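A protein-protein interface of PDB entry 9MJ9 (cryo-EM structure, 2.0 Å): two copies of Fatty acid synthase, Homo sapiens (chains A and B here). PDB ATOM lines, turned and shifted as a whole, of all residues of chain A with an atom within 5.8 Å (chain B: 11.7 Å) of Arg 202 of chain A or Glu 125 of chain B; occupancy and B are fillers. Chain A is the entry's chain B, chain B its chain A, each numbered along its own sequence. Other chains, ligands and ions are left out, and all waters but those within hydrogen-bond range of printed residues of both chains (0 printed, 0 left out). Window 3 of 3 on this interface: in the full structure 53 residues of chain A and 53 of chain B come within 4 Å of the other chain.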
ATOM      1  N   SER A 197       7.117 -25.152   5.655  1.00  0.00           N
ATOM      2  CA  SER A 197       7.090 -26.005   6.834  1.00  0.00           C
ATOM      3  C   SER A 197       5.751 -26.710   6.977  1.00  0.00           C
ATOM      4  O   SER A 197       5.697 -27.847   7.448  1.00  0.00           O
ATOM      5  CB  SER A 197       7.405 -25.186   8.078  1.00  0.00           C
ATOM      6  OG  SER A 197       8.717 -24.669   8.020  1.00  0.00           O
ATOM      7  N   VAL A 198       4.661 -26.065   6.552  1.00  0.00           N
ATOM      8  CA  VAL A 198       3.356 -26.728   6.582  1.00  0.00           C
ATOM      9  C   VAL A 198       3.312 -27.863   5.560  1.00  0.00           C
ATOM     10  O   VAL A 198       2.747 -28.932   5.824  1.00  0.00           O
ATOM     11  CB  VAL A 198       2.232 -25.698   6.368  1.00  0.00           C
ATOM     12  CG1 VAL A 198       0.885 -26.360   6.251  1.00  0.00           C
ATOM     13  CG2 VAL A 198       2.189 -24.737   7.517  1.00  0.00           C
ATOM     14  N   GLN A 199       3.941 -27.662   4.394  1.00  0.00           N
ATOM     15  CA  GLN A 199       4.059 -28.731   3.399  1.00  0.00           C
ATOM     16  C   GLN A 199       4.840 -29.923   3.939  1.00  0.00           C
ATOM     17  O   GLN A 199       4.433 -31.081   3.765  1.00  0.00           O
ATOM     18  CB  GLN A 199       4.741 -28.208   2.137  1.00  0.00           C
ATOM     19  CG  GLN A 199       3.849 -27.453   1.195  1.00  0.00           C
ATOM     20  CD  GLN A 199       4.592 -26.961  -0.024  1.00  0.00           C
ATOM     21  OE1 GLN A 199       5.773 -26.644   0.044  1.00  0.00           O
ATOM     22  NE2 GLN A 199       3.906 -26.918  -1.152  1.00  0.00           N
ATOM     23  N   PHE A 200       5.961 -29.657   4.611  1.00  0.00           N
ATOM     24  CA  PHE A 200       6.751 -30.742   5.183  1.00  0.00           C
ATOM     25  C   PHE A 200       6.027 -31.419   6.338  1.00  0.00           C
ATOM     26  O   PHE A 200       6.207 -32.619   6.560  1.00  0.00           O
ATOM     27  CB  PHE A 200       8.106 -30.223   5.646  1.00  0.00           C
ATOM     28  CG  PHE A 200       9.110 -30.115   4.547  1.00  0.00           C
ATOM     29  CD1 PHE A 200       9.487 -31.228   3.826  1.00  0.00           C
ATOM     30  CD2 PHE A 200       9.670 -28.895   4.229  1.00  0.00           C
ATOM     31  CE1 PHE A 200      10.408 -31.124   2.807  1.00  0.00           C
ATOM     32  CE2 PHE A 200      10.590 -28.786   3.215  1.00  0.00           C
ATOM     33  CZ  PHE A 200      10.960 -29.902   2.504  1.00  0.00           C
ATOM     34  N   LEU A 201       5.211 -30.672   7.080  1.00  0.00           N
ATOM     35  CA  LEU A 201       4.408 -31.260   8.145  1.00  0.00           C
ATOM     36  C   LEU A 201       3.334 -32.182   7.594  1.00  0.00           C
ATOM     37  O   LEU A 201       3.091 -33.258   8.148  1.00  0.00           O
ATOM     38  CB  LEU A 201       3.773 -30.152   8.981  1.00  0.00           C
ATOM     39  CG  LEU A 201       2.932 -30.569  10.181  1.00  0.00           C
ATOM     40  CD1 LEU A 201       3.808 -31.143  11.260  1.00  0.00           C
ATOM     41  CD2 LEU A 201       2.156 -29.387  10.692  1.00  0.00           C
ATOM     42  N   ARG A 202       2.677 -31.778   6.507  1.00  0.00           N
ATOM     43  CA  ARG A 202       1.639 -32.618   5.924  1.00  0.00           C
ATOM     44  C   ARG A 202       2.223 -33.830   5.217  1.00  0.00           C
ATOM     45  O   ARG A 202       1.540 -34.846   5.074  1.00  0.00           O
ATOM     46  CB  ARG A 202       0.784 -31.823   4.946  1.00  0.00           C
ATOM     47  CG  ARG A 202       0.038 -30.670   5.563  1.00  0.00           C
ATOM     48  CD  ARG A 202      -1.010 -31.210   6.480  1.00  0.00           C
ATOM     49  NE  ARG A 202      -1.797 -30.177   7.134  1.00  0.00           N
ATOM     50  CZ  ARG A 202      -2.860 -29.600   6.599  1.00  0.00           C
ATOM     51  NH1 ARG A 202      -3.263 -29.898   5.375  1.00  0.00           N
ATOM     52  NH2 ARG A 202      -3.545 -28.719   7.311  1.00  0.00           N
ATOM     53  N   LEU A 203       3.473 -33.745   4.757  1.00  0.00           N
ATOM     54  CA  LEU A 203       4.118 -34.928   4.200  1.00  0.00           C
ATOM     55  C   LEU A 203       4.486 -35.952   5.264  1.00  0.00           C
ATOM     56  O   LEU A 203       4.732 -37.111   4.924  1.00  0.00           O
ATOM     57  CB  LEU A 203       5.370 -34.532   3.429  1.00  0.00           C
ATOM     58  CG  LEU A 203       5.275 -34.572   1.907  1.00  0.00           C
ATOM     59  CD1 LEU A 203       6.624 -34.280   1.302  1.00  0.00           C
ATOM     60  CD2 LEU A 203       4.763 -35.914   1.445  1.00  0.00           C
ATOM     61  N   GLY A 204       4.537 -35.560   6.530  1.00  0.00           N
ATOM     62  CA  GLY A 204       4.912 -36.470   7.590  1.00  0.00           C
ATOM     63  C   GLY A 204       6.388 -36.540   7.894  1.00  0.00           C
ATOM     64  O   GLY A 204       6.825 -37.502   8.531  1.00  0.00           O
ATOM     65  N   MET A 205       7.174 -35.550   7.477  1.00  0.00           N
ATOM     66  CA  MET A 205       8.615 -35.602   7.650  1.00  0.00           C
ATOM     67  C   MET A 205       9.118 -34.840   8.865  1.00  0.00           C
ATOM     68  O   MET A 205      10.272 -35.032   9.256  1.00  0.00           O
ATOM     69  CB  MET A 205       9.318 -35.054   6.408  1.00  0.00           C
ATOM     70  CG  MET A 205       8.796 -35.610   5.112  1.00  0.00           C
ATOM     71  SD  MET A 205       9.601 -34.877   3.683  1.00  0.00           S
ATOM     72  CE  MET A 205      10.296 -36.332   2.923  1.00  0.00           C
ATOM     73  N   LYS B  70      -5.363 -38.001  -7.901  1.00  0.00           N
ATOM     74  CA  LYS B  70      -5.287 -36.898  -6.959  1.00  0.00           C
ATOM     75  C   LYS B  70      -3.889 -36.292  -6.901  1.00  0.00           C
ATOM     76  O   LYS B  70      -3.763 -35.079  -6.712  1.00  0.00           O
ATOM     77  CB  LYS B  70      -5.773 -37.399  -5.599  1.00  0.00           C
ATOM     78  CG  LYS B  70      -5.315 -36.663  -4.370  1.00  0.00           C
ATOM     79  CD  LYS B  70      -5.650 -37.465  -3.116  1.00  0.00           C
ATOM     80  CE  LYS B  70      -7.112 -37.897  -3.072  1.00  0.00           C
ATOM     81  NZ  LYS B  70      -8.054 -36.751  -3.199  1.00  0.00           N
ATOM     82  N   GLN B  71      -2.849 -37.091  -7.114  1.00  0.00           N
ATOM     83  CA  GLN B  71      -1.496 -36.576  -7.236  1.00  0.00           C
ATOM     84  C   GLN B  71      -1.231 -35.904  -8.576  1.00  0.00           C
ATOM     85  O   GLN B  71      -0.378 -35.016  -8.647  1.00  0.00           O
ATOM     86  CB  GLN B  71      -0.483 -37.702  -7.029  1.00  0.00           C
ATOM     87  CG  GLN B  71       0.717 -37.305  -6.193  1.00  0.00           C
ATOM     88  CD  GLN B  71       1.778 -36.574  -6.986  1.00  0.00           C
ATOM     89  OE1 GLN B  71       1.943 -36.805  -8.179  1.00  0.00           O
ATOM     90  NE2 GLN B  71       2.493 -35.671  -6.329  1.00  0.00           N
ATOM     91  N   THR B  74      -2.146 -32.051  -8.654  1.00  0.00           N
ATOM     92  CA  THR B  74      -1.245 -31.187  -7.911  1.00  0.00           C
ATOM     93  C   THR B  74       0.200 -31.316  -8.381  1.00  0.00           C
ATOM     94  O   THR B  74       1.127 -31.115  -7.596  1.00  0.00           O
ATOM     95  CB  THR B  74      -1.382 -31.473  -6.418  1.00  0.00           C
ATOM     96  OG1 THR B  74      -0.441 -30.684  -5.686  1.00  0.00           O
ATOM     97  CG2 THR B  74      -1.169 -32.937  -6.131  1.00  0.00           C
ATOM     98  N   ALA B 119       2.079 -21.324  -6.459  1.00  0.00           N
ATOM     99  CA  ALA B 119       0.631 -21.221  -6.586  1.00  0.00           C
ATOM    100  C   ALA B 119      -0.085 -22.265  -5.751  1.00  0.00           C
ATOM    101  O   ALA B 119      -1.187 -22.013  -5.261  1.00  0.00           O
ATOM    102  CB  ALA B 119       0.211 -21.355  -8.045  1.00  0.00           C
ATOM    103  N   LEU B 120       0.517 -23.437  -5.572  1.00  0.00           N
ATOM    104  CA  LEU B 120      -0.109 -24.526  -4.843  1.00  0.00           C
ATOM    105  C   LEU B 120       0.147 -24.466  -3.352  1.00  0.00           C
ATOM    106  O   LEU B 120      -0.374 -25.308  -2.623  1.00  0.00           O
ATOM    107  CB  LEU B 120       0.369 -25.872  -5.386  1.00  0.00           C
ATOM    108  CG  LEU B 120      -0.327 -26.371  -6.648  1.00  0.00           C
ATOM    109  CD1 LEU B 120       0.377 -27.587  -7.183  1.00  0.00           C
ATOM    110  CD2 LEU B 120      -1.774 -26.677  -6.366  1.00  0.00           C
ATOM    111  N   SER B 121       0.940 -23.506  -2.877  1.00  0.00           N
ATOM    112  CA  SER B 121       1.224 -23.381  -1.454  1.00  0.00           C
ATOM    113  C   SER B 121       0.777 -22.041  -0.889  1.00  0.00           C
ATOM    114  O   SER B 121       1.315 -21.594   0.126  1.00  0.00           O
ATOM    115  CB  SER B 121       2.710 -23.605  -1.177  1.00  0.00           C
ATOM    116  OG  SER B 121       3.505 -22.616  -1.794  1.00  0.00           O
ATOM    117  N   ARG B 122      -0.199 -21.389  -1.515  1.00  0.00           N
ATOM    118  CA  ARG B 122      -0.627 -20.081  -1.045  1.00  0.00           C
ATOM    119  C   ARG B 122      -1.558 -20.165   0.157  1.00  0.00           C
ATOM    120  O   ARG B 122      -1.602 -19.229   0.955  1.00  0.00           O
ATOM    121  CB  ARG B 122      -1.309 -19.308  -2.169  1.00  0.00           C
ATOM    122  CG  ARG B 122      -2.431 -20.043  -2.845  1.00  0.00           C
ATOM    123  CD  ARG B 122      -2.920 -19.272  -4.048  1.00  0.00           C
ATOM    124  NE  ARG B 122      -4.294 -19.601  -4.401  1.00  0.00           N
ATOM    125  CZ  ARG B 122      -4.649 -20.646  -5.133  1.00  0.00           C
ATOM    126  NH1 ARG B 122      -3.760 -21.515  -5.577  1.00  0.00           N
ATOM    127  NH2 ARG B 122      -5.933 -20.822  -5.426  1.00  0.00           N
ATOM    128  N   ASP B 123      -2.303 -21.253   0.302  1.00  0.00           N
ATOM    129  CA  ASP B 123      -3.260 -21.387   1.395  1.00  0.00           C
ATOM    130  C   ASP B 123      -2.767 -22.429   2.381  1.00  0.00           C
ATOM    131  O   ASP B 123      -2.897 -23.632   2.121  1.00  0.00           O
ATOM    132  CB  ASP B 123      -4.638 -21.775   0.859  1.00  0.00           C
ATOM    133  CG  ASP B 123      -5.744 -21.503   1.850  1.00  0.00           C
ATOM    134  OD1 ASP B 123      -5.459 -20.955   2.931  1.00  0.00           O
ATOM    135  OD2 ASP B 123      -6.905 -21.841   1.550  1.00  0.00           O
ATOM    136  N   PRO B 124      -2.243 -22.036   3.541  1.00  0.00           N
ATOM    137  CA  PRO B 124      -1.704 -23.011   4.492  1.00  0.00           C
ATOM    138  C   PRO B 124      -2.749 -23.791   5.272  1.00  0.00           C
ATOM    139  O   PRO B 124      -2.375 -24.618   6.105  1.00  0.00           O
ATOM    140  CB  PRO B 124      -0.873 -22.126   5.429  1.00  0.00           C
ATOM    141  CG  PRO B 124      -1.576 -20.841   5.414  1.00  0.00           C
ATOM    142  CD  PRO B 124      -2.068 -20.656   4.016  1.00  0.00           C
ATOM    143  N   GLU B 125      -4.036 -23.564   5.037  1.00  0.00           N
ATOM    144  CA  GLU B 125      -5.077 -24.340   5.686  1.00  0.00           C
ATOM    145  C   GLU B 125      -5.598 -25.479   4.826  1.00  0.00           C
ATOM    146  O   GLU B 125      -6.095 -26.466   5.375  1.00  0.00           O
ATOM    147  CB  GLU B 125      -6.245 -23.433   6.077  1.00  0.00           C
ATOM    148  CG  GLU B 125      -7.346 -24.148   6.827  1.00  0.00           C
ATOM    149  CD  GLU B 125      -8.464 -23.209   7.238  1.00  0.00           C
ATOM    150  OE1 GLU B 125      -8.391 -22.005   6.902  1.00  0.00           O
ATOM    151  OE2 GLU B 125      -9.419 -23.672   7.893  1.00  0.00           O
ATOM    152  N   THR B 126      -5.515 -25.366   3.501  1.00  0.00           N
ATOM    153  CA  THR B 126      -5.967 -26.401   2.581  1.00  0.00           C
ATOM    154  C   THR B 126      -4.814 -27.005   1.782  1.00  0.00           C
ATOM    155  O   THR B 126      -5.008 -27.451   0.652  1.00  0.00           O
ATOM    156  CB  THR B 126      -7.031 -25.858   1.625  1.00  0.00           C
ATOM    157  OG1 THR B 126      -6.396 -25.142   0.559  1.00  0.00           O
ATOM    158  CG2 THR B 126      -8.000 -24.943   2.337  1.00  0.00           C
ATOM    159  N   LEU B 127      -3.613 -27.014   2.351  1.00  0.00           N
ATOM    160  CA  LEU B 127      -2.469 -27.619   1.692  1.00  0.00           C
ATOM    161  C   LEU B 127      -2.581 -29.134   1.652  1.00  0.00           C
ATOM    162  O   LEU B 127      -3.282 -29.761   2.448  1.00  0.00           O
ATOM    163  CB  LEU B 127      -1.166 -27.255   2.399  1.00  0.00           C
ATOM    164  CG  LEU B 127      -0.558 -25.915   2.037  1.00  0.00           C
ATOM    165  CD1 LEU B 127       0.801 -25.740   2.627  1.00  0.00           C
ATOM    166  CD2 LEU B 127      -0.473 -25.877   0.572  1.00  0.00           C
ATOM    167  N   VAL B 128      -1.856 -29.722   0.709  1.00  0.00           N
ATOM    168  CA  VAL B 128      -1.648 -31.159   0.652  1.00  0.00           C
ATOM    169  C   VAL B 128      -0.151 -31.407   0.565  1.00  0.00           C
ATOM    170  O   VAL B 128       0.603 -30.547   0.105  1.00  0.00           O
ATOM    171  CB  VAL B 128      -2.385 -31.798  -0.538  1.00  0.00           C
ATOM    172  CG1 VAL B 128      -3.837 -31.996  -0.194  1.00  0.00           C
ATOM    173  CG2 VAL B 128      -2.242 -30.939  -1.766  1.00  0.00           C
ATOM    174  N   GLY B 129       0.278 -32.584   1.019  1.00  0.00           N
ATOM    175  CA  GLY B 129       1.690 -32.907   0.988  1.00  0.00           C
ATOM    176  C   GLY B 129       2.219 -33.260  -0.384  1.00  0.00           C
ATOM    177  O   GLY B 129       3.429 -33.166  -0.604  1.00  0.00           O
ATOM    178  N   TYR B 130       1.343 -33.641  -1.316  1.00  0.00           N
ATOM    179  CA  TYR B 130       1.793 -34.091  -2.630  1.00  0.00           C
ATOM    180  C   TYR B 130       2.321 -32.950  -3.484  1.00  0.00           C
ATOM    181  O   TYR B 130       3.006 -33.201  -4.478  1.00  0.00           O
ATOM    182  CB  TYR B 130       0.667 -34.774  -3.404  1.00  0.00           C
ATOM    183  CG  TYR B 130      -0.387 -35.454  -2.581  1.00  0.00           C
ATOM    184  CD1 TYR B 130      -0.067 -36.493  -1.718  1.00  0.00           C
ATOM    185  CD2 TYR B 130      -1.720 -35.113  -2.734  1.00  0.00           C
ATOM    186  CE1 TYR B 130      -1.042 -37.124  -0.981  1.00  0.00           C
ATOM    187  CE2 TYR B 130      -2.698 -35.731  -2.000  1.00  0.00           C
ATOM    188  CZ  TYR B 130      -2.358 -36.738  -1.128  1.00  0.00           C
ATOM    189  OH  TYR B 130      -3.341 -37.368  -0.400  1.00  0.00           O
ATOM    190  N   SER B 131       2.000 -31.706  -3.132  1.00  0.00           N
ATOM    191  CA  SER B 131       2.508 -30.574  -3.893  1.00  0.00           C
ATOM    192  C   SER B 131       4.005 -30.391  -3.697  1.00  0.00           C
ATOM    193  O   SER B 131       4.667 -29.771  -4.532  1.00  0.00           O
ATOM    194  CB  SER B 131       1.759 -29.304  -3.500  1.00  0.00           C
ATOM    195  OG  SER B 131       2.002 -28.960  -2.152  1.00  0.00           O
ATOM    196  N   MET B 132       4.557 -30.906  -2.601  1.00  0.00           N
ATOM    197  CA  MET B 132       6.003 -30.903  -2.440  1.00  0.00           C
ATOM    198  C   MET B 132       6.651 -31.918  -3.371  1.00  0.00           C
ATOM    199  O   MET B 132       7.688 -31.639  -3.979  1.00  0.00           O
ATOM    200  CB  MET B 132       6.362 -31.204  -0.988  1.00  0.00           C
ATOM    201  CG  MET B 132       7.834 -31.106  -0.666  1.00  0.00           C
ATOM    202  SD  MET B 132       8.283 -29.442  -0.151  1.00  0.00           S
ATOM    203  CE  MET B 132       9.272 -28.909  -1.537  1.00  0.00           C
ATOM    204  N   VAL B 133       6.049 -33.100  -3.499  1.00  0.00           N
ATOM    205  CA  VAL B 133       6.596 -34.165  -4.330  1.00  0.00           C
ATOM    206  C   VAL B 133       6.474 -33.855  -5.819  1.00  0.00           C
ATOM    207  O   VAL B 133       7.374 -34.197  -6.595  1.00  0.00           O
ATOM    208  CB  VAL B 133       5.903 -35.485  -3.941  1.00  0.00           C
ATOM    209  CG1 VAL B 133       6.357 -36.648  -4.798  1.00  0.00           C
ATOM    210  CG2 VAL B 133       6.160 -35.791  -2.487  1.00  0.00           C
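No position is printed for both chains. Of the 11 pairs that touch across the chains among the printed residues, none has its exchanged pair printed and touching as well.
Among the printed residues, merely in contact across the chains: Leu 203 of chain A with Gly 129 of chain B (3.4 Å), Gln 199 of chain A with Ser 121 of chain B (3.5 Å), Val 198 of chain A with Leu 127 of chain B (3.7 Å), Val 198 of chain A with Pro 124 of chain B (3.7 Å), Gln 199 of chain A with Leu 127 of chain B (3.8 Å), Phe 200 of chain A with Met 132 of chain B (3.8 Å), Leu 203 of chain A with Met 132 of chain B (3.8 Å) and Arg 202 of chain A with Glu 125 of chain B (3.9 Å).
The side-chain hydroxyl of Ser 131 of chain B is in hydrogen-bond range of the backbone carbonyl oxygen of Val 128 of chain B (3.1 Å). O of Phe 200 of chain A is in hydrogen-bond range of N of Met 205 of chain A, 3.2 Å away.
Of the 18 printed residues of chain B, 7 touch a printed residue of chain A. Of the 9 printed residues of chain A, 5 touch a printed residue of chain B. Hydrophobic or aromatic side chains of chain A within 4 Å of the printed part of chain B: Val 198, Phe 200 and Leu 203.
O of Leu 127 of chain B lies within hydrogen-bond range of NH1 of Arg 202 of chain A, 2.9 Å away. The side-chain amide nitrogen of Gln 199 of chain A sits at hydrogen-bond distance from the side-chain hydroxyl of Ser 131 of chain B (3.0 Å). The side-chain amide oxygen (OE1) of Gln 199 of chain A lies close to the side-chain sulfur (SD) of Met 132 of chain B (3.8 Å).
Arg 202 of chain A touches two residues of chain B. Of chain A, only Arg 202 (3.9 Å) comes within 4 Å of Glu 125 of chain B. No residue of chain B comes within 4 Å of Leu 201 of chain A. Of chain B, only Gly 129 (3.4 Å) and Met 132 (3.8 Å) come within 4 Å of Leu 203 of chain A. No residue of chain B comes within 4 Å of Gly 204 of chain A. Of the printed residues of chain A, Ser 121 of chain B touches Gln 199. Of the printed residues of chain A, Pro 124 of chain B touches Val 198 (3.7 Å). Of the printed residues of chain A, Ser 131 of chain B touches Gln 199. Gln 71 of chain B touches none of the printed residues of chain A. Lys 70 of chain B touches none of the printed residues of chain A.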
